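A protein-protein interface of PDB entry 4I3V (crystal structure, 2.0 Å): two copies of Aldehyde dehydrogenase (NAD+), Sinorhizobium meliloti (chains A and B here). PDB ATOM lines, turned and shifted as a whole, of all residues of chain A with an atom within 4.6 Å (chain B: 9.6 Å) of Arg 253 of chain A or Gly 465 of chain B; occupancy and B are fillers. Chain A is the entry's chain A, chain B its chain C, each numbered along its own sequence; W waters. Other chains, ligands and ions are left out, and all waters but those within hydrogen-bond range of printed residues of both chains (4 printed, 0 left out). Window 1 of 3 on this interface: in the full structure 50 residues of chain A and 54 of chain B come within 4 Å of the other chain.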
ATOM      1  N   LEU A 151       6.173  -3.640 -16.165  1.00  0.00           N
ATOM      2  CA  LEU A 151       5.412  -4.843 -15.860  1.00  0.00           C
ATOM      3  C   LEU A 151       5.820  -5.991 -16.772  1.00  0.00           C
ATOM      4  O   LEU A 151       6.645  -5.833 -17.666  1.00  0.00           O
ATOM      5  CB  LEU A 151       3.913  -4.576 -16.059  1.00  0.00           C
ATOM      6  CG  LEU A 151       3.397  -3.290 -15.406  1.00  0.00           C
ATOM      7  CD1 LEU A 151       1.914  -3.048 -15.743  1.00  0.00           C
ATOM      8  CD2 LEU A 151       3.649  -3.313 -13.885  1.00  0.00           C
ATOM      9  N   ASP A 231      -0.273  -8.249 -16.727  1.00  0.00           N
ATOM     10  CA  ASP A 231      -0.314  -7.572 -15.434  1.00  0.00           C
ATOM     11  C   ASP A 231      -1.362  -6.465 -15.408  1.00  0.00           C
ATOM     12  O   ASP A 231      -1.878  -6.107 -14.347  1.00  0.00           O
ATOM     13  CB  ASP A 231       1.052  -6.972 -15.080  1.00  0.00           C
ATOM     14  CG  ASP A 231       2.062  -8.030 -14.659  1.00  0.00           C
ATOM     15  OD1 ASP A 231       1.657  -9.193 -14.417  1.00  0.00           O
ATOM     16  OD2 ASP A 231       3.257  -7.696 -14.560  1.00  0.00           O
ATOM     17  N   LEU A 232      -1.668  -5.917 -16.575  1.00  0.00           N
ATOM     18  CA  LEU A 232      -2.574  -4.780 -16.647  1.00  0.00           C
ATOM     19  C   LEU A 232      -3.356  -4.829 -17.940  1.00  0.00           C
ATOM     20  O   LEU A 232      -2.804  -5.147 -18.989  1.00  0.00           O
ATOM     21  CB  LEU A 232      -1.793  -3.462 -16.544  1.00  0.00           C
ATOM     22  CG  LEU A 232      -2.596  -2.160 -16.440  1.00  0.00           C
ATOM     23  CD1 LEU A 232      -2.018  -1.207 -15.392  1.00  0.00           C
ATOM     24  CD2 LEU A 232      -2.620  -1.469 -17.788  1.00  0.00           C
ATOM     25  N   VAL A 233      -4.649  -4.550 -17.845  1.00  0.00           N
ATOM     26  CA  VAL A 233      -5.515  -4.415 -19.003  1.00  0.00           C
ATOM     27  C   VAL A 233      -5.941  -2.958 -19.077  1.00  0.00           C
ATOM     28  O   VAL A 233      -6.518  -2.441 -18.119  1.00  0.00           O
ATOM     29  CB  VAL A 233      -6.796  -5.271 -18.859  1.00  0.00           C
ATOM     30  CG1 VAL A 233      -7.708  -5.073 -20.074  1.00  0.00           C
ATOM     31  CG2 VAL A 233      -6.450  -6.751 -18.662  1.00  0.00           C
ATOM     32  N   TYR A 251      -7.750 -10.603 -10.878  1.00  0.00           N
ATOM     33  CA  TYR A 251      -6.744 -10.097  -9.939  1.00  0.00           C
ATOM     34  C   TYR A 251      -5.872  -9.032 -10.604  1.00  0.00           C
ATOM     35  O   TYR A 251      -5.049  -8.379  -9.956  1.00  0.00           O
ATOM     36  CB  TYR A 251      -5.923 -11.264  -9.387  1.00  0.00           C
ATOM     37  CG  TYR A 251      -4.915 -10.943  -8.294  1.00  0.00           C
ATOM     38  CD1 TYR A 251      -5.292 -10.279  -7.126  1.00  0.00           C
ATOM     39  CD2 TYR A 251      -3.595 -11.365  -8.411  1.00  0.00           C
ATOM     40  CE1 TYR A 251      -4.361 -10.013  -6.118  1.00  0.00           C
ATOM     41  CE2 TYR A 251      -2.664 -11.109  -7.415  1.00  0.00           C
ATOM     42  CZ  TYR A 251      -3.051 -10.440  -6.271  1.00  0.00           C
ATOM     43  OH  TYR A 251      -2.105 -10.184  -5.299  1.00  0.00           O
ATOM     44  N   LYS A 252      -6.102  -8.828 -11.895  1.00  0.00           N
ATOM     45  CA  LYS A 252      -5.267  -7.948 -12.700  1.00  0.00           C
ATOM     46  C   LYS A 252      -5.600  -6.467 -12.488  1.00  0.00           C
ATOM     47  O   LYS A 252      -6.742  -6.120 -12.185  1.00  0.00           O
ATOM     48  CB  LYS A 252      -5.427  -8.315 -14.174  1.00  0.00           C
ATOM     49  CG  LYS A 252      -5.337  -9.809 -14.462  1.00  0.00           C
ATOM     50  CD  LYS A 252      -5.386 -10.056 -15.979  1.00  0.00           C
ATOM     51  CE  LYS A 252      -5.096 -11.515 -16.326  1.00  0.00           C
ATOM     52  NZ  LYS A 252      -3.708 -11.900 -15.954  1.00  0.00           N
ATOM     53  N   ARG A 253      -4.604  -5.601 -12.658  1.00  0.00           N
ATOM     54  CA  ARG A 253      -4.837  -4.165 -12.655  1.00  0.00           C
ATOM     55  C   ARG A 253      -5.619  -3.833 -13.924  1.00  0.00           C
ATOM     56  O   ARG A 253      -5.389  -4.434 -14.973  1.00  0.00           O
ATOM     57  CB  ARG A 253      -3.528  -3.372 -12.695  1.00  0.00           C
ATOM     58  CG  ARG A 253      -2.584  -3.480 -11.488  1.00  0.00           C
ATOM     59  CD  ARG A 253      -1.484  -2.398 -11.628  1.00  0.00           C
ATOM     60  NE  ARG A 253      -0.130  -2.776 -11.212  1.00  0.00           N
ATOM     61  CZ  ARG A 253       0.370  -4.014 -11.187  1.00  0.00           C
ATOM     62  NH1 ARG A 253      -0.347  -5.069 -11.565  1.00  0.00           N
ATOM     63  NH2 ARG A 253       1.610  -4.205 -10.779  1.00  0.00           N
ATOM     64  N   GLN A 254      -6.517  -2.862 -13.832  1.00  0.00           N
ATOM     65  CA  GLN A 254      -7.305  -2.449 -14.978  1.00  0.00           C
ATOM     66  C   GLN A 254      -7.400  -0.944 -15.026  1.00  0.00           C
ATOM     67  O   GLN A 254      -7.513  -0.292 -13.989  1.00  0.00           O
ATOM     68  CB  GLN A 254      -8.712  -3.020 -14.881  1.00  0.00           C
ATOM     69  CG  GLN A 254      -8.781  -4.528 -14.883  1.00  0.00           C
ATOM     70  CD  GLN A 254     -10.021  -5.011 -14.156  1.00  0.00           C
ATOM     71  OE1 GLN A 254     -11.134  -4.511 -14.383  1.00  0.00           O
ATOM     72  NE2 GLN A 254      -9.834  -5.956 -13.251  1.00  0.00           N
ATOM     73  N   VAL A 255      -7.338  -0.392 -16.233  1.00  0.00           N
ATOM     74  CA  VAL A 255      -7.677   1.003 -16.435  1.00  0.00           C
ATOM     75  C   VAL A 255      -8.770   1.033 -17.503  1.00  0.00           C
ATOM     76  O   VAL A 255      -8.531   0.690 -18.655  1.00  0.00           O
ATOM     77  CB  VAL A 255      -6.456   1.855 -16.855  1.00  0.00           C
ATOM     78  CG1 VAL A 255      -6.865   3.293 -17.047  1.00  0.00           C
ATOM     79  CG2 VAL A 255      -5.321   1.753 -15.802  1.00  0.00           C
ATOM     80  N   ASN A 479       5.597  -0.451 -11.742  1.00  0.00           N
ATOM     81  CA  ASN A 479       5.567  -0.728 -10.308  1.00  0.00           C
ATOM     82  C   ASN A 479       6.585   0.167  -9.629  1.00  0.00           C
ATOM     83  O   ASN A 479       7.732   0.251 -10.081  1.00  0.00           O
ATOM     84  CB  ASN A 479       5.935  -2.196 -10.037  1.00  0.00           C
ATOM     85  CG  ASN A 479       4.839  -3.157 -10.466  1.00  0.00           C
ATOM     86  OD1 ASN A 479       3.666  -2.865 -10.293  1.00  0.00           O
ATOM     87  ND2 ASN A 479       5.219  -4.300 -11.031  1.00  0.00           N
ATOM     88  N   ALA B 246     -11.516 -10.089  -4.710  1.00  0.00           N
ATOM     89  CA  ALA B 246     -11.291  -9.582  -6.061  1.00  0.00           C
ATOM     90  C   ALA B 246     -12.381 -10.073  -7.025  1.00  0.00           C
ATOM     91  O   ALA B 246     -12.840  -9.326  -7.892  1.00  0.00           O
ATOM     92  CB  ALA B 246      -9.911  -9.977  -6.551  1.00  0.00           C
ATOM     93  N   GLN B 254     -10.194  -1.505  -5.810  1.00  0.00           N
ATOM     94  CA  GLN B 254      -9.685  -2.324  -4.721  1.00  0.00           C
ATOM     95  C   GLN B 254      -8.209  -2.066  -4.485  1.00  0.00           C
ATOM     96  O   GLN B 254      -7.413  -1.978  -5.423  1.00  0.00           O
ATOM     97  CB  GLN B 254      -9.851  -3.803  -5.052  1.00  0.00           C
ATOM     98  CG  GLN B 254     -11.249  -4.200  -5.441  1.00  0.00           C
ATOM     99  CD  GLN B 254     -11.293  -5.552  -6.116  1.00  0.00           C
ATOM    100  OE1 GLN B 254     -10.528  -6.456  -5.780  1.00  0.00           O
ATOM    101  NE2 GLN B 254     -12.189  -5.693  -7.083  1.00  0.00           N
ATOM    102  N   VAL B 255      -7.838  -1.967  -3.224  1.00  0.00           N
ATOM    103  CA  VAL B 255      -6.440  -2.040  -2.860  1.00  0.00           C
ATOM    104  C   VAL B 255      -6.285  -3.273  -2.003  1.00  0.00           C
ATOM    105  O   VAL B 255      -6.829  -3.327  -0.905  1.00  0.00           O
ATOM    106  CB  VAL B 255      -6.005  -0.800  -2.081  1.00  0.00           C
ATOM    107  CG1 VAL B 255      -4.598  -0.992  -1.536  1.00  0.00           C
ATOM    108  CG2 VAL B 255      -6.085   0.427  -2.982  1.00  0.00           C
ATOM    109  N   LEU B 256      -5.569  -4.277  -2.498  1.00  0.00           N
ATOM    110  CA  LEU B 256      -5.435  -5.522  -1.744  1.00  0.00           C
ATOM    111  C   LEU B 256      -3.993  -5.734  -1.343  1.00  0.00           C
ATOM    112  O   LEU B 256      -3.113  -5.801  -2.198  1.00  0.00           O
ATOM    113  CB  LEU B 256      -5.896  -6.719  -2.572  1.00  0.00           C
ATOM    114  CG  LEU B 256      -7.256  -6.601  -3.256  1.00  0.00           C
ATOM    115  CD1 LEU B 256      -7.539  -7.865  -4.059  1.00  0.00           C
ATOM    116  CD2 LEU B 256      -8.368  -6.338  -2.259  1.00  0.00           C
ATOM    117  N   GLU B 257      -3.749  -5.839  -0.041  1.00  0.00           N
ATOM    118  CA  GLU B 257      -2.396  -6.100   0.434  1.00  0.00           C
ATOM    119  C   GLU B 257      -2.412  -7.451   1.098  1.00  0.00           C
ATOM    120  O   GLU B 257      -3.085  -7.658   2.108  1.00  0.00           O
ATOM    121  CB  GLU B 257      -1.907  -5.009   1.391  1.00  0.00           C
ATOM    122  CG  GLU B 257      -2.149  -3.560   0.886  1.00  0.00           C
ATOM    123  CD  GLU B 257      -1.373  -3.205  -0.391  1.00  0.00           C
ATOM    124  OE1 GLU B 257      -0.596  -4.051  -0.894  1.00  0.00           O
ATOM    125  OE2 GLU B 257      -1.535  -2.064  -0.890  1.00  0.00           O
ATOM    126  N   LEU B 258      -1.676  -8.382   0.503  1.00  0.00           N
ATOM    127  CA  LEU B 258      -1.742  -9.768   0.892  1.00  0.00           C
ATOM    128  C   LEU B 258      -0.439 -10.197   1.597  1.00  0.00           C
ATOM    129  O   LEU B 258       0.307  -9.364   2.145  1.00  0.00           O
ATOM    130  CB  LEU B 258      -2.048 -10.646  -0.333  1.00  0.00           C
ATOM    131  CG  LEU B 258      -3.470 -10.669  -0.893  1.00  0.00           C
ATOM    132  CD1 LEU B 258      -4.322  -9.494  -0.451  1.00  0.00           C
ATOM    133  CD2 LEU B 258      -3.462 -10.739  -2.406  1.00  0.00           C
ATOM    134  N   GLY B 416       6.077 -11.349  -3.299  1.00  0.00           N
ATOM    135  CA  GLY B 416       6.995 -10.285  -3.661  1.00  0.00           C
ATOM    136  C   GLY B 416       6.631  -9.009  -2.932  1.00  0.00           C
ATOM    137  O   GLY B 416       5.994  -8.126  -3.490  1.00  0.00           O
ATOM    138  N   LEU B 417       7.027  -8.913  -1.672  1.00  0.00           N
ATOM    139  CA  LEU B 417       6.645  -7.762  -0.868  1.00  0.00           C
ATOM    140  C   LEU B 417       7.890  -6.955  -0.491  1.00  0.00           C
ATOM    141  O   LEU B 417       8.174  -5.939  -1.099  1.00  0.00           O
ATOM    142  CB  LEU B 417       5.858  -8.221   0.357  1.00  0.00           C
ATOM    143  CG  LEU B 417       5.232  -7.168   1.283  1.00  0.00           C
ATOM    144  CD1 LEU B 417       4.474  -6.109   0.497  1.00  0.00           C
ATOM    145  CD2 LEU B 417       4.317  -7.864   2.304  1.00  0.00           C
ATOM    146  N   GLY B 439       8.511  -5.179  -3.696  1.00  0.00           N
ATOM    147  CA  GLY B 439       8.152  -3.774  -3.580  1.00  0.00           C
ATOM    148  C   GLY B 439       9.183  -2.933  -2.841  1.00  0.00           C
ATOM    149  O   GLY B 439       9.284  -1.733  -3.081  1.00  0.00           O
ATOM    150  N   PHE B 456       4.096   1.675   0.327  1.00  0.00           N
ATOM    151  CA  PHE B 456       4.201   0.300   0.778  1.00  0.00           C
ATOM    152  C   PHE B 456       3.247  -0.570  -0.008  1.00  0.00           C
ATOM    153  O   PHE B 456       2.080  -0.224  -0.158  1.00  0.00           O
ATOM    154  CB  PHE B 456       3.853   0.211   2.267  1.00  0.00           C
ATOM    155  CG  PHE B 456       3.754  -1.197   2.780  1.00  0.00           C
ATOM    156  CD1 PHE B 456       4.896  -1.961   2.959  1.00  0.00           C
ATOM    157  CD2 PHE B 456       2.519  -1.762   3.056  1.00  0.00           C
ATOM    158  CE1 PHE B 456       4.807  -3.249   3.416  1.00  0.00           C
ATOM    159  CE2 PHE B 456       2.426  -3.056   3.515  1.00  0.00           C
ATOM    160  CZ  PHE B 456       3.577  -3.803   3.693  1.00  0.00           C
ATOM    161  N   GLY B 457       3.739  -1.695  -0.512  1.00  0.00           N
ATOM    162  CA  GLY B 457       2.891  -2.610  -1.261  1.00  0.00           C
ATOM    163  C   GLY B 457       3.737  -3.531  -2.110  1.00  0.00           C
ATOM    164  O   GLY B 457       4.813  -3.148  -2.577  1.00  0.00           O
ATOM    165  N   GLY B 458       3.252  -4.745  -2.326  1.00  0.00           N
ATOM    166  CA  GLY B 458       4.020  -5.709  -3.086  1.00  0.00           C
ATOM    167  C   GLY B 458       3.450  -6.027  -4.451  1.00  0.00           C
ATOM    168  O   GLY B 458       2.537  -5.355  -4.950  1.00  0.00           O
ATOM    169  N   ILE B 459       4.014  -7.061  -5.064  1.00  0.00           N
ATOM    170  CA  ILE B 459       3.572  -7.509  -6.372  1.00  0.00           C
ATOM    171  C   ILE B 459       3.283  -9.013  -6.315  1.00  0.00           C
ATOM    172  O   ILE B 459       3.297  -9.618  -5.233  1.00  0.00           O
ATOM    173  CB  ILE B 459       4.622  -7.175  -7.446  1.00  0.00           C
ATOM    174  CG1 ILE B 459       5.986  -7.759  -7.055  1.00  0.00           C
ATOM    175  CG2 ILE B 459       4.744  -5.651  -7.624  1.00  0.00           C
ATOM    176  CD1 ILE B 459       7.096  -7.497  -8.074  1.00  0.00           C
ATOM    177  N   LYS B 460       2.995  -9.606  -7.471  1.00  0.00           N
ATOM    178  CA  LYS B 460       2.669 -11.027  -7.544  1.00  0.00           C
ATOM    179  C   LYS B 460       1.583 -11.388  -6.526  1.00  0.00           C
ATOM    180  O   LYS B 460       0.553 -10.730  -6.481  1.00  0.00           O
ATOM    181  CB  LYS B 460       3.938 -11.865  -7.390  1.00  0.00           C
ATOM    182  CG  LYS B 460       4.982 -11.576  -8.478  1.00  0.00           C
ATOM    183  CD  LYS B 460       6.395 -11.950  -8.031  1.00  0.00           C
ATOM    184  CE  LYS B 460       6.516 -13.461  -7.832  1.00  0.00           C
ATOM    185  NZ  LYS B 460       7.910 -13.915  -7.517  1.00  0.00           N
ATOM    186  N   ASP B 461       1.772 -12.418  -5.706  1.00  0.00           N
ATOM    187  CA  ASP B 461       0.686 -12.762  -4.765  1.00  0.00           C
ATOM    188  C   ASP B 461       0.642 -11.868  -3.523  1.00  0.00           C
ATOM    189  O   ASP B 461      -0.230 -12.034  -2.671  1.00  0.00           O
ATOM    190  CB  ASP B 461       0.719 -14.228  -4.337  1.00  0.00           C
ATOM    191  CG  ASP B 461       0.040 -15.157  -5.341  1.00  0.00           C
ATOM    192  OD1 ASP B 461      -0.401 -14.684  -6.414  1.00  0.00           O
ATOM    193  OD2 ASP B 461      -0.020 -16.375  -5.057  1.00  0.00           O
ATOM    194  N   SER B 462       1.572 -10.927  -3.419  1.00  0.00           N
ATOM    195  CA  SER B 462       1.629 -10.067  -2.242  1.00  0.00           C
ATOM    196  C   SER B 462       0.629  -8.921  -2.279  1.00  0.00           C
ATOM    197  O   SER B 462       0.407  -8.252  -1.272  1.00  0.00           O
ATOM    198  CB  SER B 462       3.039  -9.531  -2.032  1.00  0.00           C
ATOM    199  OG  SER B 462       3.910 -10.592  -1.691  1.00  0.00           O
ATOM    200  N   GLY B 463       0.025  -8.689  -3.438  1.00  0.00           N
ATOM    201  CA  GLY B 463      -1.018  -7.683  -3.530  1.00  0.00           C
ATOM    202  C   GLY B 463      -1.404  -7.392  -4.960  1.00  0.00           C
ATOM    203  O   GLY B 463      -0.737  -7.845  -5.895  1.00  0.00           O
ATOM    204  N   ASN B 464      -2.473  -6.631  -5.146  1.00  0.00           N
ATOM    205  CA  ASN B 464      -2.934  -6.379  -6.505  1.00  0.00           C
ATOM    206  C   ASN B 464      -2.240  -5.211  -7.217  1.00  0.00           C
ATOM    207  O   ASN B 464      -2.669  -4.801  -8.296  1.00  0.00           O
ATOM    208  CB  ASN B 464      -4.454  -6.244  -6.557  1.00  0.00           C
ATOM    209  CG  ASN B 464      -4.963  -4.979  -5.881  1.00  0.00           C
ATOM    210  OD1 ASN B 464      -4.288  -4.392  -5.030  1.00  0.00           O
ATOM    211  ND2 ASN B 464      -6.176  -4.558  -6.254  1.00  0.00           N
ATOM    212  N   GLY B 465      -1.168  -4.686  -6.626  1.00  0.00           N
ATOM    213  CA  GLY B 465      -0.309  -3.745  -7.331  1.00  0.00           C
ATOM    214  C   GLY B 465      -0.484  -2.256  -7.056  1.00  0.00           C
ATOM    215  O   GLY B 465       0.003  -1.420  -7.824  1.00  0.00           O
ATOM    216  N   TYR B 466      -1.169  -1.917  -5.970  1.00  0.00           N
ATOM    217  CA  TYR B 466      -1.307  -0.517  -5.567  1.00  0.00           C
ATOM    218  C   TYR B 466      -0.572  -0.293  -4.254  1.00  0.00           C
ATOM    219  O   TYR B 466      -0.461  -1.194  -3.427  1.00  0.00           O
ATOM    220  CB  TYR B 466      -2.779  -0.107  -5.455  1.00  0.00           C
ATOM    221  CG  TYR B 466      -3.519  -0.319  -6.752  1.00  0.00           C
ATOM    222  CD1 TYR B 466      -3.391   0.594  -7.804  1.00  0.00           C
ATOM    223  CD2 TYR B 466      -4.297  -1.458  -6.951  1.00  0.00           C
ATOM    224  CE1 TYR B 466      -4.042   0.392  -9.004  1.00  0.00           C
ATOM    225  CE2 TYR B 466      -4.956  -1.669  -8.155  1.00  0.00           C
ATOM    226  CZ  TYR B 466      -4.823  -0.744  -9.173  1.00  0.00           C
ATOM    227  OH  TYR B 466      -5.464  -0.957 -10.366  1.00  0.00           O
ATOM    228  N   LYS B 467      -0.044   0.909  -4.080  1.00  0.00           N
ATOM    229  CA  LYS B 467       0.703   1.239  -2.880  1.00  0.00           C
ATOM    230  C   LYS B 467      -0.212   1.812  -1.806  1.00  0.00           C
ATOM    231  O   LYS B 467      -1.222   2.446  -2.096  1.00  0.00           O
ATOM    232  CB  LYS B 467       1.803   2.264  -3.199  1.00  0.00           C
ATOM    233  CG  LYS B 467       2.880   1.777  -4.159  1.00  0.00           C
ATOM    234  CD  LYS B 467       3.753   0.690  -3.518  1.00  0.00           C
ATOM    235  CE  LYS B 467       4.819   0.202  -4.482  1.00  0.00           C
ATOM    236  NZ  LYS B 467       5.765  -0.768  -3.819  1.00  0.00           N
ATOM    237  N   GLU B 468       0.156   1.587  -0.556  1.00  0.00           N
ATOM    238  CA  GLU B 468      -0.465   2.292   0.537  1.00  0.00           C
ATOM    239  C   GLU B 468       0.621   2.918   1.407  1.00  0.00           C
ATOM    240  O   GLU B 468       1.686   3.305   0.909  1.00  0.00           O
ATOM    241  CB  GLU B 468      -1.404   1.380   1.321  1.00  0.00           C
ATOM    242  CG  GLU B 468      -0.793   0.075   1.823  1.00  0.00           C
ATOM    243  CD  GLU B 468      -1.816  -0.780   2.579  1.00  0.00           C
ATOM    244  OE1 GLU B 468      -1.532  -1.220   3.726  1.00  0.00           O
ATOM    245  OE2 GLU B 468      -2.923  -0.985   2.028  1.00  0.00           O
ATOM    246  N   GLU B 472       0.271   7.522   0.047  1.00  0.00           N
ATOM    247  CA  GLU B 472      -0.339   6.840  -1.095  1.00  0.00           C
ATOM    248  C   GLU B 472      -1.795   6.453  -0.845  1.00  0.00           C
ATOM    249  O   GLU B 472      -2.621   6.467  -1.770  1.00  0.00           O
ATOM    250  CB  GLU B 472       0.501   5.640  -1.526  1.00  0.00           C
ATOM    251  CG  GLU B 472       1.855   6.040  -2.122  1.00  0.00           C
ATOM    252  CD  GLU B 472       1.718   6.839  -3.424  1.00  0.00           C
ATOM    253  OE1 GLU B 472       0.713   6.654  -4.138  1.00  0.00           O
ATOM    254  OE2 GLU B 472       2.614   7.657  -3.734  1.00  0.00           O
HETATM  255  O   HOH W   1      -2.384  -7.652  -9.706  1.00  0.00           O
HETATM  256  O   HOH W   2      -4.943   0.496 -12.540  1.00  0.00           O
HETATM  257  O   HOH W   3      -7.408  -2.487 -11.020  1.00  0.00           O
HETATM  258  O   HOH W   4       2.879  -1.662  -8.252  1.00  0.00           O
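Positions printed for both chains: 254 and 255.
The backbone carbonyl oxygen (O) of Arg 253 of chain A lies within hydrogen-bond range of the backbone NH (N) of Val 233 of chain A, at 3.0 Å. N of Leu 258 of chain B is in hydrogen-bond range of O of Ser 462 of chain B, 2.7 Å away. The guanidinium group (NH2) of Arg 253 of chain A lies within hydrogen-bond range of the side-chain amide oxygen (OD1) of Asn 479 of chain A (2.5 Å). The side-chain amide nitrogen (ND2) of Asn 464 of chain B is in hydrogen-bond range of the backbone carbonyl oxygen (O) of Gln 254 of chain B (3.0 Å). N of Leu 256 of chain B lies within hydrogen-bond range of OD1 of Asn 464 of chain B, 2.8 Å away. The backbone carbonyl oxygen (O) of Gly 416 of chain B lies within hydrogen-bond range of the backbone NH (N) of Ile 459 of chain B.
Gly 465 of chain B touches one residue of chain A. No residue of chain B comes within 4 Å of Leu 232 of chain A. Of the printed residues of chain A, Ile 459 of chain B touches Asn 479. Of the printed residues of chain B, Asn 479 of chain A touches Ile 459 (3.7 Å). Of the printed residues of chain A, Asp 461 of chain B touches Tyr 251 (3.7 Å). Of the printed residues of chain A, Asn 464 of chain B touches Tyr 251 (3.6 Å) and Arg 253 (3.5 Å). Glu 472 of chain B touches none of the printed residues of chain A. Phe 456 of chain B touches none of the printed residues of chain A. The nearest residue of chain B that does not touch Arg 253 of chain A is Ile 459 of chain B (4.7 Å). The nearest printed residue of chain B that does not touch Tyr 251 of chain A is Ser 462 of chain B (4.2 Å).
Tyr 251 of chain A touches Leu 258 of chain B (OH to CD2, 3.2 Å). Asp 461 of chain B touches Tyr 251 of chain A. Tyr 251 of chain A touches Asn 464 of chain B (OH to N, 3.6 Å). Arg 253 of chain A touches Asn 464 of chain B (CG to O, 3.5 Å). O of Gly 465 of chain B touches NE of Arg 253 of chain A, 3.7 Å away. OH of Tyr 466 of chain B touches CB of Arg 253 of chain A (3.9 Å). ND2 of Asn 479 of chain A touches CG2 of Ile 459 of chain B (3.7 Å).
Water W4 bridges OD1 of Asn 479 of chain A (2.5 Å) and O of Gly 465 of chain B (2.9 Å). Water W3 lies within hydrogen-bond range of the side-chain hydroxyl of Tyr 466 of chain B (2.6 Å) and the backbone NH of Gln 254 of chain A (3.0 Å). Water W2 lies within hydrogen-bond range of the side-chain hydroxyl (OH) of Tyr 466 of chain B (2.7 Å) and the backbone carbonyl oxygen (O) of Gln 254 of chain A (3.1 Å). Water W1 lies within hydrogen-bond range of the backbone carbonyl oxygen (O) of Tyr 251 of chain A (2.8 Å) and the backbone carbonyl oxygen (O) of Asn 464 of chain B (3.2 Å).
The backbone carbonyl oxygen (O) of Gly 463 of chain B lies within hydrogen-bond range of the side-chain hydroxyl (OH) of Tyr 251 of chain A (2.8 Å). The backbone carbonyl oxygen (O) of Lys 460 of chain B lies within hydrogen-bond range of the side-chain hydroxyl (OH) of Tyr 251 of chain A, at 3.0 Å.
Of the 10 printed residues of chain A, 3 touch a printed residue of chain B. Hydrophobic or aromatic side chains of chain A within 4 Å of the printed part of chain B: Tyr 251. Along chain A the printed residues that touch a printed residue of chain B span positions 251 to 479. Printed residues of chain B that touch a printed residue of chain A: Leu 258, Ile 459, Lys 460, Asp 461, Gly 463, Asn 464, Gly 465 and Tyr 466. Hydrophobic or aromatic side chains of chain B within 4 Å of the printed part of chain A: Leu 258, Ile 459 and Tyr 466. Among the printed residues, no Asp or Glu carboxylate lies within 4 Å of a Lys or Arg side-chain nitrogen of the other chain.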
